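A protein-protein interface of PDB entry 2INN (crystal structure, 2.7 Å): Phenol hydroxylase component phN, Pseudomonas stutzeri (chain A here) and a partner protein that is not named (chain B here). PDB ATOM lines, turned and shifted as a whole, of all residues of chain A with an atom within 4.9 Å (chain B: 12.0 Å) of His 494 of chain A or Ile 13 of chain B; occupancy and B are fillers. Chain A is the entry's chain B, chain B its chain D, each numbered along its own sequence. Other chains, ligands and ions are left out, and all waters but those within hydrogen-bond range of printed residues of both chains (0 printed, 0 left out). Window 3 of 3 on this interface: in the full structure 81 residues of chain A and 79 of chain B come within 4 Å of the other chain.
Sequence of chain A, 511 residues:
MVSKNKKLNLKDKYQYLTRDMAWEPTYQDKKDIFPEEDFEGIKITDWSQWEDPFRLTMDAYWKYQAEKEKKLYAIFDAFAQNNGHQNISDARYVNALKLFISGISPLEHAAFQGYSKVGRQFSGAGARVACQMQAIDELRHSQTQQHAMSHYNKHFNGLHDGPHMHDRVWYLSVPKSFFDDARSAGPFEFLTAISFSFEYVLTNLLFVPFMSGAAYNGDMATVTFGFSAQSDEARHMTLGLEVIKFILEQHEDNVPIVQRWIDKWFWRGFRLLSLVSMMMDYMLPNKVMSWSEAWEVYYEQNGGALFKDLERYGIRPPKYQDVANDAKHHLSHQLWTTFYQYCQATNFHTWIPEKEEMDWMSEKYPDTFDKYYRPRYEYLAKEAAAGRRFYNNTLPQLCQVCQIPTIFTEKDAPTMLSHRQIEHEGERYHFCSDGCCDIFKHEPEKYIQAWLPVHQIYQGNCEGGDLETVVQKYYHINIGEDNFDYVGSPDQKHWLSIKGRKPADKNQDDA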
ATOM      1  N   LYS A 154     -16.414  19.962   7.323  1.00  0.00           N
ATOM      2  CA  LYS A 154     -15.387  20.769   7.983  1.00  0.00           C
ATOM      3  C   LYS A 154     -15.208  22.152   7.385  1.00  0.00           C
ATOM      4  O   LYS A 154     -14.772  23.014   8.121  1.00  0.00           O
ATOM      5  CB  LYS A 154     -14.045  20.042   8.019  1.00  0.00           C
ATOM      6  CG  LYS A 154     -14.102  18.784   8.848  1.00  0.00           C
ATOM      7  CD  LYS A 154     -13.123  17.749   8.456  1.00  0.00           C
ATOM      8  CE  LYS A 154     -11.889  18.017   9.159  1.00  0.00           C
ATOM      9  NZ  LYS A 154     -11.292  16.698   9.480  1.00  0.00           N
ATOM     10  N   HIS A 155     -15.574  22.424   6.133  1.00  0.00           N
ATOM     11  CA  HIS A 155     -15.265  23.758   5.528  1.00  0.00           C
ATOM     12  C   HIS A 155     -16.475  24.628   5.096  1.00  0.00           C
ATOM     13  O   HIS A 155     -16.385  25.769   4.707  1.00  0.00           O
ATOM     14  CB  HIS A 155     -14.283  23.550   4.342  1.00  0.00           C
ATOM     15  CG  HIS A 155     -12.895  23.164   4.794  1.00  0.00           C
ATOM     16  ND1 HIS A 155     -12.561  21.877   5.201  1.00  0.00           N
ATOM     17  CD2 HIS A 155     -11.795  23.918   5.003  1.00  0.00           C
ATOM     18  CE1 HIS A 155     -11.338  21.865   5.665  1.00  0.00           C
ATOM     19  NE2 HIS A 155     -10.843  23.085   5.540  1.00  0.00           N
ATOM     20  N   ASN A 157     -20.980  25.349   5.541  1.00  0.00           N
ATOM     21  CA  ASN A 157     -22.118  25.282   6.410  1.00  0.00           C
ATOM     22  C   ASN A 157     -23.272  24.365   5.950  1.00  0.00           C
ATOM     23  O   ASN A 157     -23.375  24.012   4.806  1.00  0.00           O
ATOM     24  CB  ASN A 157     -22.529  26.677   6.739  1.00  0.00           C
ATOM     25  CG  ASN A 157     -21.482  27.393   7.605  1.00  0.00           C
ATOM     26  OD1 ASN A 157     -21.130  26.947   8.746  1.00  0.00           O
ATOM     27  ND2 ASN A 157     -21.002  28.543   7.107  1.00  0.00           N
ATOM     28  N   PRO A 490     -21.884  33.196   4.986  1.00  0.00           N
ATOM     29  CA  PRO A 490     -20.512  32.902   5.292  1.00  0.00           C
ATOM     30  C   PRO A 490     -19.862  32.014   4.231  1.00  0.00           C
ATOM     31  O   PRO A 490     -18.700  32.259   4.016  1.00  0.00           O
ATOM     32  CB  PRO A 490     -20.616  32.294   6.664  1.00  0.00           C
ATOM     33  CG  PRO A 490     -21.785  33.168   7.272  1.00  0.00           C
ATOM     34  CD  PRO A 490     -22.739  32.939   6.155  1.00  0.00           C
ATOM     35  N   ASP A 491     -20.568  31.059   3.560  1.00  0.00           N
ATOM     36  CA  ASP A 491     -19.990  30.338   2.399  1.00  0.00           C
ATOM     37  C   ASP A 491     -19.444  31.290   1.300  1.00  0.00           C
ATOM     38  O   ASP A 491     -18.259  31.206   0.882  1.00  0.00           O
ATOM     39  CB  ASP A 491     -20.947  29.335   1.737  1.00  0.00           C
ATOM     40  CG  ASP A 491     -21.097  28.015   2.527  1.00  0.00           C
ATOM     41  OD1 ASP A 491     -20.511  27.910   3.619  1.00  0.00           O
ATOM     42  OD2 ASP A 491     -21.817  27.078   2.022  1.00  0.00           O
ATOM     43  N   GLN A 492     -20.274  32.189   0.823  1.00  0.00           N
ATOM     44  CA  GLN A 492     -19.790  33.168  -0.083  1.00  0.00           C
ATOM     45  C   GLN A 492     -18.472  33.814   0.399  1.00  0.00           C
ATOM     46  O   GLN A 492     -17.575  33.936  -0.414  1.00  0.00           O
ATOM     47  CB  GLN A 492     -20.801  34.291  -0.297  1.00  0.00           C
ATOM     48  CG  GLN A 492     -20.511  35.056  -1.541  1.00  0.00           C
ATOM     49  CD  GLN A 492     -21.362  36.287  -1.740  1.00  0.00           C
ATOM     50  OE1 GLN A 492     -21.661  36.635  -2.862  1.00  0.00           O
ATOM     51  NE2 GLN A 492     -21.735  36.950  -0.689  1.00  0.00           N
ATOM     52  N   LYS A 493     -18.385  34.283   1.660  1.00  0.00           N
ATOM     53  CA  LYS A 493     -17.292  35.132   2.060  1.00  0.00           C
ATOM     54  C   LYS A 493     -16.053  34.266   1.898  1.00  0.00           C
ATOM     55  O   LYS A 493     -15.011  34.772   1.438  1.00  0.00           O
ATOM     56  CB  LYS A 493     -17.359  35.706   3.515  1.00  0.00           C
ATOM     57  CG  LYS A 493     -18.599  36.618   3.922  1.00  0.00           C
ATOM     58  CD  LYS A 493     -19.636  35.812   4.971  1.00  0.00           C
ATOM     59  CE  LYS A 493     -20.712  36.631   5.902  1.00  0.00           C
ATOM     60  NZ  LYS A 493     -20.399  38.129   5.959  1.00  0.00           N
ATOM     61  N   HIS A 494     -16.161  32.973   2.231  1.00  0.00           N
ATOM     62  CA  HIS A 494     -14.984  32.148   2.351  1.00  0.00           C
ATOM     63  C   HIS A 494     -14.560  31.798   0.983  1.00  0.00           C
ATOM     64  O   HIS A 494     -13.462  32.178   0.555  1.00  0.00           O
ATOM     65  CB  HIS A 494     -15.191  30.910   3.182  1.00  0.00           C
ATOM     66  CG  HIS A 494     -15.703  31.222   4.549  1.00  0.00           C
ATOM     67  ND1 HIS A 494     -16.326  30.283   5.360  1.00  0.00           N
ATOM     68  CD2 HIS A 494     -15.741  32.398   5.230  1.00  0.00           C
ATOM     69  CE1 HIS A 494     -16.686  30.863   6.495  1.00  0.00           C
ATOM     70  NE2 HIS A 494     -16.342  32.142   6.442  1.00  0.00           N
ATOM     71  N   TRP A 495     -15.400  31.112   0.252  1.00  0.00           N
ATOM     72  CA  TRP A 495     -15.028  30.882  -1.130  1.00  0.00           C
ATOM     73  C   TRP A 495     -14.297  32.060  -1.847  1.00  0.00           C
ATOM     74  O   TRP A 495     -13.125  31.915  -2.310  1.00  0.00           O
ATOM     75  CB  TRP A 495     -16.278  30.539  -1.896  1.00  0.00           C
ATOM     76  CG  TRP A 495     -16.015  30.052  -3.226  1.00  0.00           C
ATOM     77  CD1 TRP A 495     -16.310  30.676  -4.393  1.00  0.00           C
ATOM     78  CD2 TRP A 495     -15.429  28.818  -3.559  1.00  0.00           C
ATOM     79  NE1 TRP A 495     -15.991  29.873  -5.447  1.00  0.00           N
ATOM     80  CE2 TRP A 495     -15.398  28.743  -4.973  1.00  0.00           C
ATOM     81  CE3 TRP A 495     -14.939  27.768  -2.816  1.00  0.00           C
ATOM     82  CZ2 TRP A 495     -14.863  27.684  -5.656  1.00  0.00           C
ATOM     83  CZ3 TRP A 495     -14.435  26.683  -3.504  1.00  0.00           C
ATOM     84  CH2 TRP A 495     -14.406  26.649  -4.920  1.00  0.00           C
ATOM     85  N   LEU A 496     -14.994  33.195  -1.935  1.00  0.00           N
ATOM     86  CA  LEU A 496     -14.470  34.374  -2.553  1.00  0.00           C
ATOM     87  C   LEU A 496     -13.069  34.718  -2.143  1.00  0.00           C
ATOM     88  O   LEU A 496     -12.318  35.245  -2.983  1.00  0.00           O
ATOM     89  CB  LEU A 496     -15.343  35.590  -2.367  1.00  0.00           C
ATOM     90  CG  LEU A 496     -16.511  35.532  -3.354  1.00  0.00           C
ATOM     91  CD1 LEU A 496     -17.373  36.850  -3.307  1.00  0.00           C
ATOM     92  CD2 LEU A 496     -16.217  35.074  -4.838  1.00  0.00           C
ATOM     93  N   SER A 497     -12.671  34.445  -0.908  1.00  0.00           N
ATOM     94  CA  SER A 497     -11.265  34.682  -0.557  1.00  0.00           C
ATOM     95  C   SER A 497     -10.223  33.504  -1.005  1.00  0.00           C
ATOM     96  O   SER A 497      -9.558  32.839  -0.197  1.00  0.00           O
ATOM     97  CB  SER A 497     -11.228  35.081   0.911  1.00  0.00           C
ATOM     98  OG  SER A 497     -11.769  34.001   1.610  1.00  0.00           O
ATOM     99  N   ILE A 498     -10.163  33.275  -2.324  1.00  0.00           N
ATOM    100  CA  ILE A 498      -9.363  32.302  -3.085  1.00  0.00           C
ATOM    101  C   ILE A 498      -9.975  32.380  -4.547  1.00  0.00           C
ATOM    102  O   ILE A 498     -10.847  31.581  -5.067  1.00  0.00           O
ATOM    103  CB  ILE A 498      -9.288  30.902  -2.403  1.00  0.00           C
ATOM    104  CG1 ILE A 498     -10.471  30.645  -1.438  1.00  0.00           C
ATOM    105  CG2 ILE A 498      -7.858  30.759  -1.656  1.00  0.00           C
ATOM    106  CD1 ILE A 498     -11.037  29.196  -1.375  1.00  0.00           C
ATOM    107  N   SER B   9      -2.013  24.172   4.447  1.00  0.00           N
ATOM    108  CA  SER B   9      -3.228  23.866   5.222  1.00  0.00           C
ATOM    109  C   SER B   9      -4.383  24.917   5.115  1.00  0.00           C
ATOM    110  O   SER B   9      -4.279  25.956   4.389  1.00  0.00           O
ATOM    111  CB  SER B   9      -2.958  23.333   6.651  1.00  0.00           C
ATOM    112  OG  SER B   9      -2.415  24.320   7.498  1.00  0.00           O
ATOM    113  N   VAL B  10      -5.502  24.561   5.753  1.00  0.00           N
ATOM    114  CA  VAL B  10      -6.721  25.386   5.734  1.00  0.00           C
ATOM    115  C   VAL B  10      -7.271  25.353   7.170  1.00  0.00           C
ATOM    116  O   VAL B  10      -7.205  24.299   7.833  1.00  0.00           O
ATOM    117  CB  VAL B  10      -7.803  24.928   4.663  1.00  0.00           C
ATOM    118  CG1 VAL B  10      -8.987  25.908   4.624  1.00  0.00           C
ATOM    119  CG2 VAL B  10      -7.181  24.792   3.257  1.00  0.00           C
ATOM    120  N   GLU B  11      -7.737  26.516   7.650  1.00  0.00           N
ATOM    121  CA  GLU B  11      -8.469  26.568   8.863  1.00  0.00           C
ATOM    122  C   GLU B  11      -9.849  25.998   8.594  1.00  0.00           C
ATOM    123  O   GLU B  11     -10.537  26.426   7.669  1.00  0.00           O
ATOM    124  CB  GLU B  11      -8.536  27.982   9.370  1.00  0.00           C
ATOM    125  CG  GLU B  11      -7.551  28.194  10.501  1.00  0.00           C
ATOM    126  CD  GLU B  11      -7.999  27.558  11.862  1.00  0.00           C
ATOM    127  OE1 GLU B  11      -7.502  28.007  12.938  1.00  0.00           O
ATOM    128  OE2 GLU B  11      -8.845  26.615  11.865  1.00  0.00           O
ATOM    129  N   PRO B  12     -10.230  24.974   9.354  1.00  0.00           N
ATOM    130  CA  PRO B  12     -11.566  24.407   9.171  1.00  0.00           C
ATOM    131  C   PRO B  12     -12.578  25.118  10.072  1.00  0.00           C
ATOM    132  O   PRO B  12     -12.258  25.400  11.247  1.00  0.00           O
ATOM    133  CB  PRO B  12     -11.383  22.955   9.663  1.00  0.00           C
ATOM    134  CG  PRO B  12     -10.387  23.078  10.788  1.00  0.00           C
ATOM    135  CD  PRO B  12      -9.471  24.273  10.409  1.00  0.00           C
ATOM    136  N   ILE B  13     -13.765  25.379   9.549  1.00  0.00           N
ATOM    137  CA  ILE B  13     -14.871  25.827  10.383  1.00  0.00           C
ATOM    138  C   ILE B  13     -15.213  24.921  11.631  1.00  0.00           C
ATOM    139  O   ILE B  13     -15.299  25.410  12.780  1.00  0.00           O
ATOM    140  CB  ILE B  13     -16.086  25.973   9.538  1.00  0.00           C
ATOM    141  CG1 ILE B  13     -16.021  27.267   8.763  1.00  0.00           C
ATOM    142  CG2 ILE B  13     -17.308  26.069  10.391  1.00  0.00           C
ATOM    143  CD1 ILE B  13     -17.494  27.803   8.468  1.00  0.00           C
ATOM    144  N   ARG B  14     -15.398  23.611  11.417  1.00  0.00           N
ATOM    145  CA  ARG B  14     -15.400  22.681  12.555  1.00  0.00           C
ATOM    146  C   ARG B  14     -14.688  21.371  12.308  1.00  0.00           C
ATOM    147  O   ARG B  14     -14.210  21.101  11.243  1.00  0.00           O
ATOM    148  CB  ARG B  14     -16.801  22.411  13.001  1.00  0.00           C
ATOM    149  CG  ARG B  14     -17.629  21.665  12.014  1.00  0.00           C
ATOM    150  CD  ARG B  14     -18.986  22.350  11.870  1.00  0.00           C
ATOM    151  NE  ARG B  14     -19.105  22.665  10.469  1.00  0.00           N
ATOM    152  CZ  ARG B  14     -19.716  23.747   9.988  1.00  0.00           C
ATOM    153  NH1 ARG B  14     -20.327  24.602  10.813  1.00  0.00           N
ATOM    154  NH2 ARG B  14     -19.748  23.952   8.673  1.00  0.00           N
ATOM    155  N   HIS B  15     -14.622  20.535  13.322  1.00  0.00           N
ATOM    156  CA  HIS B  15     -13.821  19.353  13.128  1.00  0.00           C
ATOM    157  C   HIS B  15     -14.575  18.132  12.780  1.00  0.00           C
ATOM    158  O   HIS B  15     -14.058  17.256  12.106  1.00  0.00           O
ATOM    159  CB  HIS B  15     -12.964  19.077  14.380  1.00  0.00           C
ATOM    160  CG  HIS B  15     -11.851  20.047  14.499  1.00  0.00           C
ATOM    161  ND1 HIS B  15     -11.670  20.842  15.625  1.00  0.00           N
ATOM    162  CD2 HIS B  15     -10.931  20.443  13.563  1.00  0.00           C
ATOM    163  CE1 HIS B  15     -10.659  21.663  15.384  1.00  0.00           C
ATOM    164  NE2 HIS B  15     -10.223  21.463  14.132  1.00  0.00           N
ATOM    165  N   THR B  16     -15.775  18.031  13.334  1.00  0.00           N
ATOM    166  CA  THR B  16     -16.638  16.924  12.978  1.00  0.00           C
ATOM    167  C   THR B  16     -18.113  17.406  12.739  1.00  0.00           C
ATOM    168  O   THR B  16     -18.330  18.606  12.539  1.00  0.00           O
ATOM    169  CB  THR B  16     -16.454  15.827  14.013  1.00  0.00           C
ATOM    170  OG1 THR B  16     -17.052  14.630  13.516  1.00  0.00           O
ATOM    171  CG2 THR B  16     -17.053  16.213  15.332  1.00  0.00           C
ATOM    172  N   TYR B  17     -19.064  16.472  12.765  1.00  0.00           N
ATOM    173  CA  TYR B  17     -20.458  16.733  12.830  1.00  0.00           C
ATOM    174  C   TYR B  17     -20.982  16.879  14.251  1.00  0.00           C
ATOM    175  O   TYR B  17     -20.363  16.376  15.210  1.00  0.00           O
ATOM    176  CB  TYR B  17     -21.169  15.543  12.298  1.00  0.00           C
ATOM    177  CG  TYR B  17     -20.821  15.171  10.836  1.00  0.00           C
ATOM    178  CD1 TYR B  17     -20.155  13.969  10.534  1.00  0.00           C
ATOM    179  CD2 TYR B  17     -21.264  15.965   9.778  1.00  0.00           C
ATOM    180  CE1 TYR B  17     -19.913  13.557   9.246  1.00  0.00           C
ATOM    181  CE2 TYR B  17     -21.045  15.565   8.446  1.00  0.00           C
ATOM    182  CZ  TYR B  17     -20.329  14.361   8.181  1.00  0.00           C
ATOM    183  OH  TYR B  17     -20.067  14.008   6.862  1.00  0.00           O
ATOM    184  N   GLY B  18     -22.180  17.513  14.382  1.00  0.00           N
ATOM    185  CA  GLY B  18     -22.778  17.912  15.662  1.00  0.00           C
ATOM    186  C   GLY B  18     -23.099  16.718  16.495  1.00  0.00           C
ATOM    187  O   GLY B  18     -22.859  16.716  17.705  1.00  0.00           O
ATOM    188  N   ALA B  21     -19.474  15.665  17.516  1.00  0.00           N
ATOM    189  CA  ALA B  21     -19.065  16.688  18.479  1.00  0.00           C
ATOM    190  C   ALA B  21     -19.834  16.616  19.836  1.00  0.00           C
ATOM    191  O   ALA B  21     -19.237  16.799  20.860  1.00  0.00           O
ATOM    192  CB  ALA B  21     -19.137  18.097  17.880  1.00  0.00           C
ATOM    193  N   GLY B  25     -16.737  15.380  21.578  1.00  0.00           N
ATOM    194  CA  GLY B  25     -16.101  16.637  21.828  1.00  0.00           C
ATOM    195  C   GLY B  25     -15.807  17.252  20.515  1.00  0.00           C
ATOM    196  O   GLY B  25     -15.886  16.550  19.533  1.00  0.00           O
ATOM    197  N   ASP B  26     -15.426  18.530  20.478  1.00  0.00           N
ATOM    198  CA  ASP B  26     -15.169  19.223  19.229  1.00  0.00           C
ATOM    199  C   ASP B  26     -13.759  18.967  18.566  1.00  0.00           C
ATOM    200  O   ASP B  26     -13.067  19.858  18.012  1.00  0.00           O
ATOM    201  CB  ASP B  26     -15.507  20.723  19.416  1.00  0.00           C
ATOM    202  CG  ASP B  26     -15.435  21.552  18.079  1.00  0.00           C
ATOM    203  OD1 ASP B  26     -15.591  21.033  16.886  1.00  0.00           O
ATOM    204  OD2 ASP B  26     -15.231  22.785  18.264  1.00  0.00           O
ATOM    205  N   LYS B  27     -13.313  17.744  18.564  1.00  0.00           N
ATOM    206  CA  LYS B  27     -12.011  17.540  17.988  1.00  0.00           C
ATOM    207  C   LYS B  27     -12.221  16.689  16.729  1.00  0.00           C
ATOM    208  O   LYS B  27     -13.298  16.110  16.599  1.00  0.00           O
ATOM    209  CB  LYS B  27     -11.201  16.802  19.026  1.00  0.00           C
ATOM    210  CG  LYS B  27     -11.711  15.406  19.258  1.00  0.00           C
ATOM    211  CD  LYS B  27     -11.655  15.029  20.706  1.00  0.00           C
ATOM    212  CE  LYS B  27     -11.313  13.588  20.880  1.00  0.00           C
ATOM    213  NZ  LYS B  27     -11.118  13.624  22.376  1.00  0.00           N
ATOM    214  N   PRO B  28     -11.208  16.522  15.863  1.00  0.00           N
ATOM    215  CA  PRO B  28     -11.476  15.588  14.763  1.00  0.00           C
ATOM    216  C   PRO B  28     -11.765  14.208  15.333  1.00  0.00           C
ATOM    217  O   PRO B  28     -11.198  13.887  16.365  1.00  0.00           O
ATOM    218  CB  PRO B  28     -10.139  15.510  13.997  1.00  0.00           C
ATOM    219  CG  PRO B  28      -9.382  16.705  14.412  1.00  0.00           C
ATOM    220  CD  PRO B  28      -9.812  17.023  15.832  1.00  0.00           C
ATOM    221  N   GLU B  34     -17.578   8.632  12.954  1.00  0.00           N
ATOM    222  CA  GLU B  34     -18.461   9.183  11.964  1.00  0.00           C
ATOM    223  C   GLU B  34     -19.335   8.105  11.242  1.00  0.00           C
ATOM    224  O   GLU B  34     -20.338   8.424  10.618  1.00  0.00           O
ATOM    225  CB  GLU B  34     -17.659  10.056  11.016  1.00  0.00           C
ATOM    226  CG  GLU B  34     -16.917  11.127  11.768  1.00  0.00           C
ATOM    227  CD  GLU B  34     -16.288  12.199  10.851  1.00  0.00           C
ATOM    228  OE1 GLU B  34     -16.133  11.907   9.633  1.00  0.00           O
ATOM    229  OE2 GLU B  34     -15.901  13.326  11.336  1.00  0.00           O
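The backbone NH (N) of Ile 13 of chain B sits at hydrogen-bond distance from the backbone carbonyl oxygen (O) of Lys 154 of chain A, at 2.9 Å. The backbone carbonyl oxygen (O) of Lys 154 of chain A is in hydrogen-bond range of the backbone NH (N) of Arg 14 of chain B, at 3.4 Å. The side-chain amide oxygen of Asn 157 of chain A is in hydrogen-bond range of the guanidinium group of Arg 14 of chain B (3.2 Å).
OD1 of Asp 491 of chain A lies within hydrogen-bond range of N of Asn 157 of chain A (3.2 Å). O of Pro 490 of chain A lies close to ND1 of His 494 of chain A (3.4 Å). The side-chain hydroxyl of Ser 497 of chain A lies within hydrogen-bond range of the backbone carbonyl oxygen of His 494 of chain A (2.7 Å). The backbone carbonyl oxygen (O) of Asp 26 of chain B lies within hydrogen-bond range of a ring nitrogen (ND1) of His 15 of chain B (2.9 Å).
Among the printed residues, merely in contact across the chains: Lys 154 of chain A with Pro 12 of chain B (3.6 Å), Lys 154 of chain A with His 15 of chain B (3.6 Å), His 155 of chain A with Val 10 of chain B (3.5 Å), His 155 of chain A with Glu 11 of chain B (3.9 Å), His 155 of chain A with Pro 12 of chain B (3.9 Å), Asn 157 of chain A with Ile 13 of chain B (3.7 Å) and His 494 of chain A with Ile 13 of chain B (3.7 Å).
His 494 of chain A touches one residue of chain B. Ile 13 of chain B touches three residues of chain A. His 155 of chain A touches just these residues of chain B: Val 10, Glu 11 and Pro 12. No residue of chain B comes within 4 Å of Asp 491 of chain A. No residue of chain B comes within 4 Å of Lys 493 of chain A. No residue of chain B comes within 4 Å of Trp 495 of chain A. No residue of chain B comes within 4 Å of Leu 496 of chain A. No residue of chain B comes within 4 Å of Ser 497 of chain A. Ile 498 of chain A touches none of the printed residues of chain B. Of the printed residues of chain A, Pro 12 of chain B touches Lys 154 and His 155. Of the printed residues of chain A, Val 10 of chain B touches His 155 (3.5 Å). Printed residues of chain A within 4 Å of Arg 14 of chain B: Lys 154 (3.3 Å) and Asn 157 (3.2 Å). Asp 26 of chain B touches none of the printed residues of chain A. The nearest residue of chain B that does not touch His 494 of chain A is Glu 11 of chain B (7.3 Å). The nearest residue of chain A that does not touch Ile 13 of chain B is His 155 of chain A (4.3 Å). The nearest printed residue of chain A that does not touch Pro 12 of chain B is His 494 of chain A (7.9 Å).
Of the 16 printed residues of chain B, 6 touch a printed residue of chain A. Printed residues of chain B that touch a printed residue of chain A: Val 10, Glu 11, Pro 12, Ile 13, Arg 14 and His 15. Hydrophobic or aromatic side chains of chain B within 4 Å of the printed part of chain A: Val 10, Pro 12 and Ile 13. Printed residues of chain A that touch a printed residue of chain B: Lys 154, His 155, Asn 157 and His 494. Hydrophobic or aromatic side chains of chain A that line the printed part of chain B: His 155 and His 494. Among the printed residues, 10 pairs touch across the chains. Among the printed residues, no Asp or Glu carboxylate lies within 4 Å of a Lys or Arg side-chain nitrogen of the other chain.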
